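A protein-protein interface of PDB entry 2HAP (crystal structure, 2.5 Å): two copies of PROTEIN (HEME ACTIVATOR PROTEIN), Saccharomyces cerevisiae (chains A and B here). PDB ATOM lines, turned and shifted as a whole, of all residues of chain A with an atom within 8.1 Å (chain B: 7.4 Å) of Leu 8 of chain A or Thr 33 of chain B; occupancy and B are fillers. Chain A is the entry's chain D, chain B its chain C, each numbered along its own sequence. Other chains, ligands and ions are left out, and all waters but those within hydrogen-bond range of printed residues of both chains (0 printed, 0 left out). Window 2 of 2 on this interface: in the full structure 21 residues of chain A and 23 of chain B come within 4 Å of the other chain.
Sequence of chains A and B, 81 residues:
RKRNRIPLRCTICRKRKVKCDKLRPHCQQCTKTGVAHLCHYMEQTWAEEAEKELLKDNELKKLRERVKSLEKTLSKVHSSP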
ATOM      1  N   ARG A   5      20.270   7.148   4.009  1.00  0.00           N
ATOM      2  CA  ARG A   5      19.227   7.069   5.021  1.00  0.00           C
ATOM      3  C   ARG A   5      18.237   8.200   4.818  1.00  0.00           C
ATOM      4  O   ARG A   5      18.639   9.356   4.753  1.00  0.00           O
ATOM      5  CB  ARG A   5      19.852   7.197   6.403  1.00  0.00           C
ATOM      6  CG  ARG A   5      19.182   6.392   7.497  1.00  0.00           C
ATOM      7  CD  ARG A   5      19.825   6.740   8.812  1.00  0.00           C
ATOM      8  NE  ARG A   5      19.016   6.372   9.962  1.00  0.00           N
ATOM      9  CZ  ARG A   5      19.509   6.242  11.188  1.00  0.00           C
ATOM     10  NH1 ARG A   5      20.810   6.453  11.408  1.00  0.00           N
ATOM     11  NH2 ARG A   5      18.701   5.911  12.192  1.00  0.00           N
ATOM     12  N   ILE A   6      16.955   7.876   4.712  1.00  0.00           N
ATOM     13  CA  ILE A   6      15.936   8.899   4.527  1.00  0.00           C
ATOM     14  C   ILE A   6      15.113   8.987   5.801  1.00  0.00           C
ATOM     15  O   ILE A   6      14.639   7.984   6.313  1.00  0.00           O
ATOM     16  CB  ILE A   6      15.014   8.575   3.331  1.00  0.00           C
ATOM     17  CG1 ILE A   6      15.847   8.469   2.055  1.00  0.00           C
ATOM     18  CG2 ILE A   6      13.992   9.675   3.144  1.00  0.00           C
ATOM     19  CD1 ILE A   6      15.361   7.408   1.097  1.00  0.00           C
ATOM     20  N   PRO A   7      14.916  10.207   6.315  1.00  0.00           N
ATOM     21  CA  PRO A   7      14.147  10.389   7.544  1.00  0.00           C
ATOM     22  C   PRO A   7      12.873   9.569   7.596  1.00  0.00           C
ATOM     23  O   PRO A   7      12.189   9.414   6.597  1.00  0.00           O
ATOM     24  CB  PRO A   7      13.850  11.880   7.563  1.00  0.00           C
ATOM     25  CG  PRO A   7      14.980  12.492   6.803  1.00  0.00           C
ATOM     26  CD  PRO A   7      15.356  11.494   5.741  1.00  0.00           C
ATOM     27  N   LEU A   8      12.554   9.034   8.763  1.00  0.00           N
ATOM     28  CA  LEU A   8      11.328   8.271   8.900  1.00  0.00           C
ATOM     29  C   LEU A   8      10.286   9.121   9.629  1.00  0.00           C
ATOM     30  O   LEU A   8       9.126   8.731   9.793  1.00  0.00           O
ATOM     31  CB  LEU A   8      11.608   6.957   9.634  1.00  0.00           C
ATOM     32  CG  LEU A   8      12.126   5.811   8.728  1.00  0.00           C
ATOM     33  CD1 LEU A   8      12.945   4.831   9.547  1.00  0.00           C
ATOM     34  CD2 LEU A   8      10.958   5.072   8.055  1.00  0.00           C
ATOM     35  N   ARG A   9      10.718  10.306  10.053  1.00  0.00           N
ATOM     36  CA  ARG A   9       9.842  11.257  10.735  1.00  0.00           C
ATOM     37  C   ARG A   9       9.208  12.112   9.647  1.00  0.00           C
ATOM     38  O   ARG A   9       9.774  12.248   8.559  1.00  0.00           O
ATOM     39  CB  ARG A   9      10.645  12.214  11.628  1.00  0.00           C
ATOM     40  CG  ARG A   9      11.421  11.603  12.787  1.00  0.00           C
ATOM     41  CD  ARG A   9      12.009  12.678  13.705  1.00  0.00           C
ATOM     42  NE  ARG A   9      13.072  13.453  13.055  1.00  0.00           N
ATOM     43  CZ  ARG A   9      13.854  14.319  13.696  1.00  0.00           C
ATOM     44  NH1 ARG A   9      13.690  14.520  15.003  1.00  0.00           N
ATOM     45  NH2 ARG A   9      14.797  14.990  13.044  1.00  0.00           N
ATOM     46  N   CYS A  10       8.036  12.699   9.914  1.00  0.00           N
ATOM     47  CA  CYS A  10       7.426  13.562   8.911  1.00  0.00           C
ATOM     48  C   CYS A  10       8.344  14.774   8.826  1.00  0.00           C
ATOM     49  O   CYS A  10       8.873  15.239   9.829  1.00  0.00           O
ATOM     50  CB  CYS A  10       6.027  13.986   9.300  1.00  0.00           C
ATOM     51  SG  CYS A  10       6.066  15.224  10.601  1.00  0.00           S
ATOM     52  N   THR A  11       8.510  15.299   7.623  1.00  0.00           N
ATOM     53  CA  THR A  11       9.419  16.414   7.374  1.00  0.00           C
ATOM     54  C   THR A  11       9.170  17.674   8.190  1.00  0.00           C
ATOM     55  O   THR A  11      10.090  18.478   8.373  1.00  0.00           O
ATOM     56  CB  THR A  11       9.398  16.833   5.906  1.00  0.00           C
ATOM     57  OG1 THR A  11       8.198  17.567   5.661  1.00  0.00           O
ATOM     58  CG2 THR A  11       9.454  15.625   4.983  1.00  0.00           C
ATOM     59  N   ARG A  14      10.531  17.189  11.942  1.00  0.00           N
ATOM     60  CA  ARG A  14      11.847  16.605  11.820  1.00  0.00           C
ATOM     61  C   ARG A  14      12.672  17.882  11.805  1.00  0.00           C
ATOM     62  O   ARG A  14      13.844  17.905  12.165  1.00  0.00           O
ATOM     63  CB  ARG A  14      11.965  15.883  10.480  1.00  0.00           C
ATOM     64  CG  ARG A  14      13.346  15.348  10.159  1.00  0.00           C
ATOM     65  CD  ARG A  14      14.267  16.416   9.612  1.00  0.00           C
ATOM     66  NE  ARG A  14      14.629  16.190   8.213  1.00  0.00           N
ATOM     67  CZ  ARG A  14      15.778  15.658   7.807  1.00  0.00           C
ATOM     68  NH1 ARG A  14      16.700  15.284   8.695  1.00  0.00           N
ATOM     69  NH2 ARG A  14      16.011  15.517   6.509  1.00  0.00           N
ATOM     70  N   CYS A  20       8.535  12.303  16.448  1.00  0.00           N
ATOM     71  CA  CYS A  20       7.445  12.057  15.534  1.00  0.00           C
ATOM     72  C   CYS A  20       6.756  10.711  15.735  1.00  0.00           C
ATOM     73  O   CYS A  20       7.376   9.654  15.631  1.00  0.00           O
ATOM     74  CB  CYS A  20       7.916  12.149  14.076  1.00  0.00           C
ATOM     75  SG  CYS A  20       6.515  11.997  12.900  1.00  0.00           S
ATOM     76  N   ASP A  21       5.471  10.751  16.040  1.00  0.00           N
ATOM     77  CA  ASP A  21       4.701   9.521  16.164  1.00  0.00           C
ATOM     78  C   ASP A  21       4.376   9.360  14.694  1.00  0.00           C
ATOM     79  O   ASP A  21       3.502  10.052  14.185  1.00  0.00           O
ATOM     80  CB  ASP A  21       3.424   9.774  16.956  1.00  0.00           C
ATOM     81  CG  ASP A  21       2.577  10.881  16.362  1.00  0.00           C
ATOM     82  OD1 ASP A  21       3.033  12.054  16.353  1.00  0.00           O
ATOM     83  OD2 ASP A  21       1.459  10.573  15.897  1.00  0.00           O
ATOM     84  N   LYS A  22       5.072   8.473  13.993  1.00  0.00           N
ATOM     85  CA  LYS A  22       4.869   8.332  12.550  1.00  0.00           C
ATOM     86  C   LYS A  22       3.506   7.861  12.053  1.00  0.00           C
ATOM     87  O   LYS A  22       3.421   7.033  11.136  1.00  0.00           O
ATOM     88  CB  LYS A  22       5.953   7.428  11.987  1.00  0.00           C
ATOM     89  CG  LYS A  22       7.335   8.035  12.033  1.00  0.00           C
ATOM     90  CD  LYS A  22       8.112   7.511  13.223  1.00  0.00           C
ATOM     91  CE  LYS A  22       8.486   6.064  13.018  1.00  0.00           C
ATOM     92  NZ  LYS A  22       8.775   5.387  14.304  1.00  0.00           N
ATOM     93  N   LEU A  23       2.447   8.386  12.660  1.00  0.00           N
ATOM     94  CA  LEU A  23       1.066   8.052  12.306  1.00  0.00           C
ATOM     95  C   LEU A  23       0.740   8.531  10.884  1.00  0.00           C
ATOM     96  O   LEU A  23       1.261   9.552  10.443  1.00  0.00           O
ATOM     97  CB  LEU A  23       0.142   8.729  13.306  1.00  0.00           C
ATOM     98  CG  LEU A  23      -1.346   8.731  12.994  1.00  0.00           C
ATOM     99  CD1 LEU A  23      -1.857   7.311  13.118  1.00  0.00           C
ATOM    100  CD2 LEU A  23      -2.091   9.688  13.947  1.00  0.00           C
ATOM    101  N   ARG A  24      -0.142   7.819  10.176  1.00  0.00           N
ATOM    102  CA  ARG A  24      -0.465   8.189   8.797  1.00  0.00           C
ATOM    103  C   ARG A  24      -1.948   8.401   8.545  1.00  0.00           C
ATOM    104  O   ARG A  24      -2.794   7.729   9.141  1.00  0.00           O
ATOM    105  CB  ARG A  24       0.048   7.127   7.846  1.00  0.00           C
ATOM    106  CG  ARG A  24       1.423   6.678   8.153  1.00  0.00           C
ATOM    107  CD  ARG A  24       2.379   7.204   7.122  1.00  0.00           C
ATOM    108  NE  ARG A  24       3.755   6.961   7.512  1.00  0.00           N
ATOM    109  CZ  ARG A  24       4.748   6.813   6.648  1.00  0.00           C
ATOM    110  NH1 ARG A  24       4.506   6.883   5.349  1.00  0.00           N
ATOM    111  NH2 ARG A  24       5.977   6.576   7.075  1.00  0.00           N
ATOM    112  N   CYS A  27       1.001  12.608  11.319  1.00  0.00           N
ATOM    113  CA  CYS A  27       1.384  12.406  12.705  1.00  0.00           C
ATOM    114  C   CYS A  27       0.599  13.297  13.681  1.00  0.00           C
ATOM    115  O   CYS A  27       0.341  14.469  13.413  1.00  0.00           O
ATOM    116  CB  CYS A  27       2.889  12.666  12.850  1.00  0.00           C
ATOM    117  SG  CYS A  27       3.376  14.406  13.043  1.00  0.00           S
ATOM    118  N   HIS A  40       3.786  15.181   5.842  1.00  0.00           N
ATOM    119  CA  HIS A  40       4.031  14.167   4.844  1.00  0.00           C
ATOM    120  C   HIS A  40       5.378  13.529   5.148  1.00  0.00           C
ATOM    121  O   HIS A  40       6.212  14.139   5.817  1.00  0.00           O
ATOM    122  CB  HIS A  40       3.989  14.782   3.428  1.00  0.00           C
ATOM    123  CG  HIS A  40       5.105  15.737   3.128  1.00  0.00           C
ATOM    124  ND1 HIS A  40       4.942  17.106   3.145  1.00  0.00           N
ATOM    125  CD2 HIS A  40       6.389  15.518   2.758  1.00  0.00           C
ATOM    126  CE1 HIS A  40       6.070  17.692   2.800  1.00  0.00           C
ATOM    127  NE2 HIS A  40       6.965  16.751   2.557  1.00  0.00           N
ATOM    128  N   TYR A  41       5.572  12.300   4.681  1.00  0.00           N
ATOM    129  CA  TYR A  41       6.817  11.574   4.923  1.00  0.00           C
ATOM    130  C   TYR A  41       7.580  11.373   3.626  1.00  0.00           C
ATOM    131  O   TYR A  41       6.985  11.080   2.602  1.00  0.00           O
ATOM    132  CB  TYR A  41       6.508  10.215   5.554  1.00  0.00           C
ATOM    133  CG  TYR A  41       5.643  10.293   6.788  1.00  0.00           C
ATOM    134  CD1 TYR A  41       4.258  10.402   6.688  1.00  0.00           C
ATOM    135  CD2 TYR A  41       6.219  10.324   8.060  1.00  0.00           C
ATOM    136  CE1 TYR A  41       3.462  10.524   7.831  1.00  0.00           C
ATOM    137  CE2 TYR A  41       5.436  10.443   9.215  1.00  0.00           C
ATOM    138  CZ  TYR A  41       4.066  10.556   9.095  1.00  0.00           C
ATOM    139  OH  TYR A  41       3.299  10.692  10.239  1.00  0.00           O
ATOM    140  N   MET A  42       8.894  11.543   3.679  1.00  0.00           N
ATOM    141  CA  MET A  42       9.769  11.374   2.522  1.00  0.00           C
ATOM    142  C   MET A  42       9.771   9.945   1.988  1.00  0.00           C
ATOM    143  O   MET A  42       9.680   8.991   2.757  1.00  0.00           O
ATOM    144  CB  MET A  42      11.195  11.758   2.896  1.00  0.00           C
ATOM    145  CG  MET A  42      11.378  13.232   3.197  1.00  0.00           C
ATOM    146  SD  MET A  42      13.120  13.623   3.443  1.00  0.00           S
ATOM    147  CE  MET A  42      13.043  15.353   3.816  1.00  0.00           C
ATOM    148  N   GLN A  44      10.941   6.424   0.721  1.00  0.00           N
ATOM    149  CA  GLN A  44      12.068   5.528   0.952  1.00  0.00           C
ATOM    150  C   GLN A  44      12.331   4.723  -0.321  1.00  0.00           C
ATOM    151  O   GLN A  44      11.400   4.415  -1.060  1.00  0.00           O
ATOM    152  CB  GLN A  44      11.754   4.562   2.096  1.00  0.00           C
ATOM    153  CG  GLN A  44      11.307   5.230   3.369  1.00  0.00           C
ATOM    154  CD  GLN A  44      12.444   5.900   4.094  1.00  0.00           C
ATOM    155  OE1 GLN A  44      13.531   5.342   4.216  1.00  0.00           O
ATOM    156  NE2 GLN A  44      12.203   7.110   4.579  1.00  0.00           N
ATOM    157  N   TRP A  46      13.218   1.702  -0.417  1.00  0.00           N
ATOM    158  CA  TRP A  46      12.748   0.333  -0.239  1.00  0.00           C
ATOM    159  C   TRP A  46      11.235   0.173  -0.182  1.00  0.00           C
ATOM    160  O   TRP A  46      10.734  -0.943  -0.011  1.00  0.00           O
ATOM    161  CB  TRP A  46      13.396  -0.304   1.000  1.00  0.00           C
ATOM    162  CG  TRP A  46      13.511   0.564   2.208  1.00  0.00           C
ATOM    163  CD1 TRP A  46      14.641   1.155   2.669  1.00  0.00           C
ATOM    164  CD2 TRP A  46      12.476   0.891   3.147  1.00  0.00           C
ATOM    165  NE1 TRP A  46      14.382   1.829   3.832  1.00  0.00           N
ATOM    166  CE2 TRP A  46      13.060   1.682   4.149  1.00  0.00           C
ATOM    167  CE3 TRP A  46      11.111   0.589   3.238  1.00  0.00           C
ATOM    168  CZ2 TRP A  46      12.340   2.173   5.224  1.00  0.00           C
ATOM    169  CZ3 TRP A  46      10.392   1.081   4.314  1.00  0.00           C
ATOM    170  CH2 TRP A  46      11.012   1.863   5.290  1.00  0.00           C
ATOM    171  N   ILE B  12       8.651  -5.678   2.662  1.00  0.00           N
ATOM    172  CA  ILE B  12       9.453  -4.517   3.061  1.00  0.00           C
ATOM    173  C   ILE B  12      10.713  -4.982   3.781  1.00  0.00           C
ATOM    174  O   ILE B  12      11.803  -4.444   3.563  1.00  0.00           O
ATOM    175  CB  ILE B  12       8.673  -3.568   4.003  1.00  0.00           C
ATOM    176  CG1 ILE B  12       7.617  -2.812   3.203  1.00  0.00           C
ATOM    177  CG2 ILE B  12       9.619  -2.551   4.656  1.00  0.00           C
ATOM    178  CD1 ILE B  12       8.184  -1.784   2.265  1.00  0.00           C
ATOM    179  N   ARG B  16      14.445  -4.300   2.746  1.00  0.00           N
ATOM    180  CA  ARG B  16      15.328  -3.696   3.738  1.00  0.00           C
ATOM    181  C   ARG B  16      16.384  -4.628   4.298  1.00  0.00           C
ATOM    182  O   ARG B  16      17.188  -4.204   5.126  1.00  0.00           O
ATOM    183  CB  ARG B  16      14.510  -3.195   4.901  1.00  0.00           C
ATOM    184  CG  ARG B  16      14.719  -1.774   5.177  1.00  0.00           C
ATOM    185  CD  ARG B  16      13.403  -1.194   5.515  1.00  0.00           C
ATOM    186  NE  ARG B  16      12.962  -1.713   6.788  1.00  0.00           N
ATOM    187  CZ  ARG B  16      13.556  -1.437   7.941  1.00  0.00           C
ATOM    188  NH1 ARG B  16      14.613  -0.644   7.975  1.00  0.00           N
ATOM    189  NH2 ARG B  16      13.075  -1.941   9.065  1.00  0.00           N
ATOM    190  N   CYS B  27       3.938  -6.908  10.094  1.00  0.00           N
ATOM    191  CA  CYS B  27       5.060  -7.199  10.967  1.00  0.00           C
ATOM    192  C   CYS B  27       5.370  -5.934  11.772  1.00  0.00           C
ATOM    193  O   CYS B  27       5.114  -4.816  11.315  1.00  0.00           O
ATOM    194  CB  CYS B  27       6.265  -7.616  10.144  1.00  0.00           C
ATOM    195  SG  CYS B  27       7.125  -6.188   9.480  1.00  0.00           S
ATOM    196  N   GLN B  28       5.951  -6.127  12.952  1.00  0.00           N
ATOM    197  CA  GLN B  28       6.272  -5.045  13.868  1.00  0.00           C
ATOM    198  C   GLN B  28       7.460  -4.194  13.427  1.00  0.00           C
ATOM    199  O   GLN B  28       7.638  -3.066  13.895  1.00  0.00           O
ATOM    200  CB  GLN B  28       6.520  -5.627  15.255  1.00  0.00           C
ATOM    201  CG  GLN B  28       6.700  -4.594  16.328  1.00  0.00           C
ATOM    202  CD  GLN B  28       5.384  -4.086  16.852  1.00  0.00           C
ATOM    203  OE1 GLN B  28       4.423  -4.847  16.983  1.00  0.00           O
ATOM    204  NE2 GLN B  28       5.329  -2.790  17.155  1.00  0.00           N
ATOM    205  N   GLN B  29       8.275  -4.721  12.517  1.00  0.00           N
ATOM    206  CA  GLN B  29       9.419  -3.969  12.025  1.00  0.00           C
ATOM    207  C   GLN B  29       8.825  -2.793  11.281  1.00  0.00           C
ATOM    208  O   GLN B  29       9.169  -1.646  11.552  1.00  0.00           O
ATOM    209  CB  GLN B  29      10.263  -4.809  11.074  1.00  0.00           C
ATOM    210  CG  GLN B  29      11.100  -5.882  11.764  1.00  0.00           C
ATOM    211  CD  GLN B  29      10.271  -6.835  12.654  1.00  0.00           C
ATOM    212  OE1 GLN B  29       9.255  -7.392  12.232  1.00  0.00           O
ATOM    213  NE2 GLN B  29      10.716  -7.021  13.890  1.00  0.00           N
ATOM    214  N   CYS B  30       7.905  -3.077  10.362  1.00  0.00           N
ATOM    215  CA  CYS B  30       7.249  -2.037   9.582  1.00  0.00           C
ATOM    216  C   CYS B  30       6.487  -1.070  10.478  1.00  0.00           C
ATOM    217  O   CYS B  30       6.602   0.143  10.314  1.00  0.00           O
ATOM    218  CB  CYS B  30       6.270  -2.648   8.556  1.00  0.00           C
ATOM    219  SG  CYS B  30       7.069  -3.416   7.100  1.00  0.00           S
ATOM    220  N   THR B  31       5.718  -1.591  11.430  1.00  0.00           N
ATOM    221  CA  THR B  31       4.969  -0.699  12.319  1.00  0.00           C
ATOM    222  C   THR B  31       5.896   0.275  13.043  1.00  0.00           C
ATOM    223  O   THR B  31       5.565   1.442  13.211  1.00  0.00           O
ATOM    224  CB  THR B  31       4.144  -1.462  13.382  1.00  0.00           C
ATOM    225  OG1 THR B  31       3.271  -2.412  12.749  1.00  0.00           O
ATOM    226  CG2 THR B  31       3.300  -0.483  14.173  1.00  0.00           C
ATOM    227  N   LYS B  32       7.071  -0.190  13.453  1.00  0.00           N
ATOM    228  CA  LYS B  32       7.975   0.705  14.157  1.00  0.00           C
ATOM    229  C   LYS B  32       8.518   1.791  13.245  1.00  0.00           C
ATOM    230  O   LYS B  32       8.560   2.950  13.634  1.00  0.00           O
ATOM    231  CB  LYS B  32       9.129  -0.073  14.781  1.00  0.00           C
ATOM    232  CG  LYS B  32       8.671  -1.127  15.791  1.00  0.00           C
ATOM    233  CD  LYS B  32       8.160  -0.512  17.092  1.00  0.00           C
ATOM    234  CE  LYS B  32       8.706  -1.274  18.296  1.00  0.00           C
ATOM    235  NZ  LYS B  32       8.541  -2.747  18.089  1.00  0.00           N
ATOM    236  N   THR B  33       8.938   1.427  12.039  1.00  0.00           N
ATOM    237  CA  THR B  33       9.462   2.412  11.099  1.00  0.00           C
ATOM    238  C   THR B  33       8.321   3.252  10.530  1.00  0.00           C
ATOM    239  O   THR B  33       8.542   4.150   9.720  1.00  0.00           O
ATOM    240  CB  THR B  33      10.182   1.735   9.929  1.00  0.00           C
ATOM    241  OG1 THR B  33       9.276   0.845   9.279  1.00  0.00           O
ATOM    242  CG2 THR B  33      11.392   0.966  10.426  1.00  0.00           C
ATOM    243  N   GLY B  34       7.098   2.949  10.955  1.00  0.00           N
ATOM    244  CA  GLY B  34       5.928   3.677  10.474  1.00  0.00           C
ATOM    245  C   GLY B  34       5.313   3.319   9.118  1.00  0.00           C
ATOM    246  O   GLY B  34       4.293   3.903   8.753  1.00  0.00           O
ATOM    247  N   VAL B  35       5.891   2.373   8.377  1.00  0.00           N
ATOM    248  CA  VAL B  35       5.365   2.004   7.056  1.00  0.00           C
ATOM    249  C   VAL B  35       4.516   0.737   7.070  1.00  0.00           C
ATOM    250  O   VAL B  35       4.725  -0.141   6.245  1.00  0.00           O
ATOM    251  CB  VAL B  35       6.518   1.797   6.024  1.00  0.00           C
ATOM    252  CG1 VAL B  35       7.284   3.097   5.822  1.00  0.00           C
ATOM    253  CG2 VAL B  35       7.471   0.691   6.488  1.00  0.00           C
ATOM    254  N   ALA B  36       3.545   0.654   7.972  1.00  0.00           N
ATOM    255  CA  ALA B  36       2.715  -0.533   8.086  1.00  0.00           C
ATOM    256  C   ALA B  36       1.714  -0.703   6.958  1.00  0.00           C
ATOM    257  O   ALA B  36       1.388  -1.830   6.558  1.00  0.00           O
ATOM    258  CB  ALA B  36       1.992  -0.517   9.418  1.00  0.00           C
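The side-chain amino group of Lys 22 of chain A is in hydrogen-bond range of the backbone carbonyl oxygen of Lys 32 of chain B (2.5 Å).
The backbone carbonyl oxygen of Gly 34 of chain B is in hydrogen-bond range of the guanidinium group of Arg 24 of chain A, 3.3 Å away.
The side-chain amide nitrogen (NE2) of Gln 28 of chain B sits close to the side-chain amino group (NZ) of Lys 32 of chain B (3.3 Å).
The backbone carbonyl oxygen (O) of Gln 29 of chain B lies within hydrogen-bond range of the side-chain hydroxyl (OG1) of Thr 33 of chain B (3.4 Å).
O of Cys 30 of chain B is in hydrogen-bond range of OG1 of Thr 33 of chain B, at 3.0 Å.
N of Val 35 of chain B sits at hydrogen-bond distance from O of Cys 30 of chain B.
Leu 8 of chain A touches Thr 33 of chain B.
Lys 22 of chain A touches Thr 33 of chain B (CE to C, 3.8 Å).
Lys 22 of chain A touches Gly 34 of chain B.
Arg 24 of chain A touches Val 35 of chain B.
Trp 46 of chain A touches Ile 12 of chain B.
Arg 16 of chain B touches Trp 46 of chain A.
CG2 of Val 35 of chain B touches CZ3 of Trp 46 of chain A, at 3.7 Å.
Printed residues of chain B within 4 Å of Leu 8 of chain A: Thr 33.
Thr 33 of chain B touches two residues of chain A.
Of the printed residues of chain B, Arg 24 of chain A touches Gly 34 and Val 35.
Printed residues of chain B within 4 Å of Trp 46 of chain A: Ile 12, Arg 16 and Val 35.
Gln 29 of chain B touches none of the printed residues of chain A.
Met 42 of chain A touches none of the printed residues of chain B.
The nearest residue of chain A that does not touch Thr 33 of chain B is Arg 24 of chain A (4.4 Å).
The nearest printed residue of chain A that does not touch Ile 12 of chain B is Gln 44 of chain A (7.3 Å).
Printed residues of chain A that touch a printed residue of chain B: Leu 8, Lys 22, Arg 24 and Trp 46.
Of the 12 printed residues of chain B, 6 touch a printed residue of chain A.
Along chain B the printed residues that touch a printed residue of chain A span positions 12 to 35.
Among the printed residues, no Asp or Glu carboxylate lies within 4 Å of a Lys or Arg side-chain nitrogen of the other chain.
Position printed for both chains: 27.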
